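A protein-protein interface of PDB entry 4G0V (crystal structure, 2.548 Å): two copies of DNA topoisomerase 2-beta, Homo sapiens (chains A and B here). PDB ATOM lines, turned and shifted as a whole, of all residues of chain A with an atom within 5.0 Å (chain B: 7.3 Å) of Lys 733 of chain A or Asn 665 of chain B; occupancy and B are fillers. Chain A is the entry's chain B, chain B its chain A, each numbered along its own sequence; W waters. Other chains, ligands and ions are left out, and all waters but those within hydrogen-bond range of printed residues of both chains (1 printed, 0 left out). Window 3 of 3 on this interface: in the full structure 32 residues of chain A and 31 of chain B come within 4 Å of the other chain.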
ATOM      1  N   ILE A 657      12.916  23.985 -15.704  1.00  0.00           N
ATOM      2  CA  ILE A 657      13.313  23.376 -14.444  1.00  0.00           C
ATOM      3  C   ILE A 657      12.866  24.204 -13.249  1.00  0.00           C
ATOM      4  O   ILE A 657      13.082  23.805 -12.106  1.00  0.00           O
ATOM      5  CB  ILE A 657      14.851  23.138 -14.345  1.00  0.00           C
ATOM      6  CG1 ILE A 657      15.607  24.458 -14.209  1.00  0.00           C
ATOM      7  CG2 ILE A 657      15.379  22.328 -15.541  1.00  0.00           C
ATOM      8  CD1 ILE A 657      17.112  24.280 -14.138  1.00  0.00           C
ATOM      9  N   LEU A 731      17.010  18.456 -19.219  1.00  0.00           N
ATOM     10  CA  LEU A 731      16.466  19.017 -17.994  1.00  0.00           C
ATOM     11  C   LEU A 731      17.264  18.569 -16.783  1.00  0.00           C
ATOM     12  O   LEU A 731      16.982  18.990 -15.667  1.00  0.00           O
ATOM     13  CB  LEU A 731      15.002  18.624 -17.837  1.00  0.00           C
ATOM     14  CG  LEU A 731      14.091  18.977 -19.018  1.00  0.00           C
ATOM     15  CD1 LEU A 731      12.658  18.523 -18.762  1.00  0.00           C
ATOM     16  CD2 LEU A 731      14.137  20.481 -19.296  1.00  0.00           C
ATOM     17  N   THR A 732      18.270  17.727 -17.000  1.00  0.00           N
ATOM     18  CA  THR A 732      19.008  17.150 -15.877  1.00  0.00           C
ATOM     19  C   THR A 732      20.189  18.029 -15.479  1.00  0.00           C
ATOM     20  O   THR A 732      20.720  18.780 -16.306  1.00  0.00           O
ATOM     21  CB  THR A 732      19.482  15.692 -16.152  1.00  0.00           C
ATOM     22  OG1 THR A 732      20.547  15.691 -17.106  1.00  0.00           O
ATOM     23  CG2 THR A 732      18.343  14.845 -16.672  1.00  0.00           C
ATOM     24  N   LYS A 733      20.595  17.915 -14.214  1.00  0.00           N
ATOM     25  CA  LYS A 733      21.593  18.806 -13.625  1.00  0.00           C
ATOM     26  C   LYS A 733      22.807  19.024 -14.523  1.00  0.00           C
ATOM     27  O   LYS A 733      23.105  20.159 -14.898  1.00  0.00           O
ATOM     28  CB  LYS A 733      22.035  18.317 -12.238  1.00  0.00           C
ATOM     29  CG  LYS A 733      23.069  19.229 -11.575  1.00  0.00           C
ATOM     30  CD  LYS A 733      23.366  18.845 -10.135  1.00  0.00           C
ATOM     31  CE  LYS A 733      22.097  18.838  -9.278  1.00  0.00           C
ATOM     32  NZ  LYS A 733      21.489  20.193  -9.125  1.00  0.00           N
ATOM     33  N   GLU A 734      23.482  17.938 -14.891  1.00  0.00           N
ATOM     34  CA  GLU A 734      24.703  18.032 -15.681  1.00  0.00           C
ATOM     35  C   GLU A 734      24.469  18.678 -17.044  1.00  0.00           C
ATOM     36  O   GLU A 734      25.298  19.443 -17.521  1.00  0.00           O
ATOM     37  CB  GLU A 734      25.367  16.661 -15.838  1.00  0.00           C
ATOM     38  CG  GLU A 734      25.922  16.070 -14.542  1.00  0.00           C
ATOM     39  CD  GLU A 734      24.879  15.316 -13.739  1.00  0.00           C
ATOM     40  OE1 GLU A 734      23.734  15.179 -14.222  1.00  0.00           O
ATOM     41  OE2 GLU A 734      25.198  14.860 -12.620  1.00  0.00           O
ATOM     42  N   LYS A 735      23.334  18.388 -17.667  1.00  0.00           N
ATOM     43  CA  LYS A 735      23.069  18.937 -18.992  1.00  0.00           C
ATOM     44  C   LYS A 735      22.718  20.430 -18.950  1.00  0.00           C
ATOM     45  O   LYS A 735      23.009  21.170 -19.885  1.00  0.00           O
ATOM     46  CB  LYS A 735      21.982  18.132 -19.703  1.00  0.00           C
ATOM     47  CG  LYS A 735      22.447  16.764 -20.186  1.00  0.00           C
ATOM     48  CD  LYS A 735      23.551  16.892 -21.200  1.00  0.00           C
ATOM     49  CE  LYS A 735      23.926  15.558 -21.793  1.00  0.00           C
ATOM     50  NZ  LYS A 735      25.001  15.725 -22.810  1.00  0.00           N
ATOM     51  N   VAL A 736      22.095  20.865 -17.857  1.00  0.00           N
ATOM     52  CA  VAL A 736      21.803  22.277 -17.651  1.00  0.00           C
ATOM     53  C   VAL A 736      23.092  23.105 -17.534  1.00  0.00           C
ATOM     54  O   VAL A 736      23.241  24.130 -18.197  1.00  0.00           O
ATOM     55  CB  VAL A 736      20.921  22.489 -16.406  1.00  0.00           C
ATOM     56  CG1 VAL A 736      20.796  23.974 -16.083  1.00  0.00           C
ATOM     57  CG2 VAL A 736      19.556  21.870 -16.629  1.00  0.00           C
ATOM     58  N   GLU A 737      24.022  22.647 -16.703  1.00  0.00           N
ATOM     59  CA  GLU A 737      25.316  23.308 -16.574  1.00  0.00           C
ATOM     60  C   GLU A 737      26.083  23.275 -17.888  1.00  0.00           C
ATOM     61  O   GLU A 737      26.685  24.269 -18.281  1.00  0.00           O
ATOM     62  CB  GLU A 737      26.150  22.671 -15.457  1.00  0.00           C
ATOM     63  CG  GLU A 737      25.477  22.723 -14.097  1.00  0.00           C
ATOM     64  CD  GLU A 737      26.070  21.745 -13.094  1.00  0.00           C
ATOM     65  OE1 GLU A 737      26.985  20.972 -13.469  1.00  0.00           O
ATOM     66  OE2 GLU A 737      25.610  21.751 -11.926  1.00  0.00           O
ATOM     67  N   THR B 662       9.443  13.580 -11.655  1.00  0.00           N
ATOM     68  CA  THR B 662      10.095  14.763 -12.200  1.00  0.00           C
ATOM     69  C   THR B 662      11.582  14.513 -12.410  1.00  0.00           C
ATOM     70  O   THR B 662      12.243  13.900 -11.576  1.00  0.00           O
ATOM     71  CB  THR B 662       9.929  15.988 -11.292  1.00  0.00           C
ATOM     72  OG1 THR B 662      10.500  15.705 -10.011  1.00  0.00           O
ATOM     73  CG2 THR B 662       8.471  16.335 -11.138  1.00  0.00           C
ATOM     74  N   ILE B 663      12.105  14.990 -13.533  1.00  0.00           N
ATOM     75  CA  ILE B 663      13.520  14.840 -13.824  1.00  0.00           C
ATOM     76  C   ILE B 663      14.240  16.187 -13.711  1.00  0.00           C
ATOM     77  O   ILE B 663      15.468  16.227 -13.602  1.00  0.00           O
ATOM     78  CB  ILE B 663      13.743  14.208 -15.225  1.00  0.00           C
ATOM     79  CG1 ILE B 663      13.376  15.188 -16.340  1.00  0.00           C
ATOM     80  CG2 ILE B 663      12.909  12.957 -15.377  1.00  0.00           C
ATOM     81  CD1 ILE B 663      13.418  14.570 -17.732  1.00  0.00           C
ATOM     82  N   GLU B 664      13.464  17.275 -13.710  1.00  0.00           N
ATOM     83  CA  GLU B 664      14.007  18.640 -13.707  1.00  0.00           C
ATOM     84  C   GLU B 664      15.115  18.871 -12.686  1.00  0.00           C
ATOM     85  O   GLU B 664      14.899  18.782 -11.485  1.00  0.00           O
ATOM     86  CB  GLU B 664      12.901  19.678 -13.519  1.00  0.00           C
ATOM     87  CG  GLU B 664      12.052  19.951 -14.764  1.00  0.00           C
ATOM     88  CD  GLU B 664      11.010  18.869 -15.022  1.00  0.00           C
ATOM     89  OE1 GLU B 664      11.032  17.842 -14.303  1.00  0.00           O
ATOM     90  OE2 GLU B 664      10.165  19.048 -15.935  1.00  0.00           O
ATOM     91  N   ASN B 665      16.310  19.135 -13.198  1.00  0.00           N
ATOM     92  CA  ASN B 665      17.478  19.475 -12.397  1.00  0.00           C
ATOM     93  C   ASN B 665      17.962  18.396 -11.427  1.00  0.00           C
ATOM     94  O   ASN B 665      18.663  18.696 -10.458  1.00  0.00           O
ATOM     95  CB  ASN B 665      17.282  20.822 -11.689  1.00  0.00           C
ATOM     96  CG  ASN B 665      18.596  21.513 -11.386  1.00  0.00           C
ATOM     97  OD1 ASN B 665      18.901  21.806 -10.232  1.00  0.00           O
ATOM     98  ND2 ASN B 665      19.395  21.750 -12.420  1.00  0.00           N
ATOM     99  N   ARG B 666      17.620  17.139 -11.702  1.00  0.00           N
ATOM    100  CA  ARG B 666      18.179  16.022 -10.940  1.00  0.00           C
ATOM    101  C   ARG B 666      19.471  15.540 -11.566  1.00  0.00           C
ATOM    102  O   ARG B 666      19.646  15.624 -12.776  1.00  0.00           O
ATOM    103  CB  ARG B 666      17.188  14.876 -10.863  1.00  0.00           C
ATOM    104  CG  ARG B 666      15.840  15.305 -10.348  1.00  0.00           C
ATOM    105  CD  ARG B 666      14.900  14.136 -10.297  1.00  0.00           C
ATOM    106  NE  ARG B 666      15.165  13.264  -9.162  1.00  0.00           N
ATOM    107  CZ  ARG B 666      14.278  13.006  -8.210  1.00  0.00           C
ATOM    108  NH1 ARG B 666      13.067  13.557  -8.266  1.00  0.00           N
ATOM    109  NH2 ARG B 666      14.598  12.195  -7.210  1.00  0.00           N
ATOM    110  N   SER B 667      20.389  15.044 -10.747  1.00  0.00           N
ATOM    111  CA  SER B 667      21.663  14.586 -11.278  1.00  0.00           C
ATOM    112  C   SER B 667      21.443  13.270 -11.991  1.00  0.00           C
ATOM    113  O   SER B 667      20.453  12.579 -11.733  1.00  0.00           O
ATOM    114  CB  SER B 667      22.694  14.414 -10.168  1.00  0.00           C
ATOM    115  OG  SER B 667      22.249  13.483  -9.205  1.00  0.00           O
ATOM    116  N   LYS B 668      22.364  12.929 -12.884  1.00  0.00           N
ATOM    117  CA  LYS B 668      22.268  11.700 -13.653  1.00  0.00           C
ATOM    118  C   LYS B 668      22.034  10.496 -12.733  1.00  0.00           C
ATOM    119  O   LYS B 668      21.094   9.713 -12.942  1.00  0.00           O
ATOM    120  CB  LYS B 668      23.529  11.511 -14.491  1.00  0.00           C
ATOM    121  CG  LYS B 668      23.450  10.385 -15.497  1.00  0.00           C
ATOM    122  CD  LYS B 668      24.654  10.414 -16.412  1.00  0.00           C
ATOM    123  CE  LYS B 668      24.622   9.286 -17.426  1.00  0.00           C
ATOM    124  NZ  LYS B 668      25.608   9.503 -18.527  1.00  0.00           N
ATOM    125  N   ASP B 670      20.968  10.396  -9.551  1.00  0.00           N
ATOM    126  CA  ASP B 670      19.665  10.443  -8.906  1.00  0.00           C
ATOM    127  C   ASP B 670      18.611   9.940  -9.856  1.00  0.00           C
ATOM    128  O   ASP B 670      17.671   9.265  -9.451  1.00  0.00           O
ATOM    129  CB  ASP B 670      19.292  11.868  -8.506  1.00  0.00           C
ATOM    130  CG  ASP B 670      20.065  12.358  -7.314  1.00  0.00           C
ATOM    131  OD1 ASP B 670      20.727  11.528  -6.648  1.00  0.00           O
ATOM    132  OD2 ASP B 670      20.003  13.580  -7.046  1.00  0.00           O
HETATM  133  O   HOH W   1      25.135  12.223 -11.727  1.00  0.00           O
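Among the printed residues, merely in contact across the chains: Ile 657 of chain A with Glu 664 of chain B, Ile 657 of chain A with Asn 665 of chain B, Leu 731 of chain A with Ile 663 of chain B, Leu 731 of chain A with Glu 664 of chain B, Thr 732 of chain A with Arg 666 of chain B, Lys 733 of chain A with Ser 667 of chain B and Glu 734 of chain A with Ser 667 of chain B.
Printed residues of chain A that touch a printed residue of chain B: Ile 657, Leu 731, Thr 732, Lys 733 and Glu 734.
Hydrophobic or aromatic side chains of chain A within 4 Å of the printed part of chain B: Ile 657 and Leu 731.
Of the 8 printed residues of chain B, 6 touch a printed residue of chain A.
Water W1 lies within hydrogen-bond range of OE2 of Glu 734 of chain A and N of Lys 668 of chain B.
The backbone carbonyl oxygen of Thr 662 of chain B lies close to the guanidinium group of Arg 666 of chain B (3.4 Å).
The side-chain hydroxyl (OG) of Ser 667 of chain B lies close to the side-chain carboxylate (OD2) of Asp 670 of chain B.
No position is printed for both chains.
The backbone NH of Asn 665 of chain B lies within hydrogen-bond range of the backbone carbonyl oxygen of Leu 731 of chain A (2.6 Å).
The side-chain amino group (NZ) of Lys 733 of chain A sits at hydrogen-bond distance from the side-chain amide oxygen (OD1) of Asn 665 of chain B (3.2 Å).
The backbone carbonyl oxygen of Arg 666 of chain B sits at hydrogen-bond distance from the backbone NH of Lys 733 of chain A, at 2.9 Å.
N of Lys 668 of chain B lies within hydrogen-bond range of OE1 of Glu 734 of chain A, 3.0 Å away.
Asn 665 of chain B touches just these residues of chain A: Ile 657, Leu 731 and Lys 733.
Printed residues of chain A within 4 Å of Arg 666 of chain B: Thr 732 and Lys 733.
Of the printed residues of chain A, Ser 667 of chain B touches Lys 733 and Glu 734.
Asp 670 of chain B touches none of the printed residues of chain A.
The nearest printed residue of chain B that does not touch Lys 733 of chain A is Ile 663 of chain B (5.4 Å).
The nearest residue of chain A that does not touch Asn 665 of chain B is Val 736 of chain A (4.2 Å).
The nearest printed residue of chain B that does not touch Thr 732 of chain A is Asn 665 of chain B (4.3 Å).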
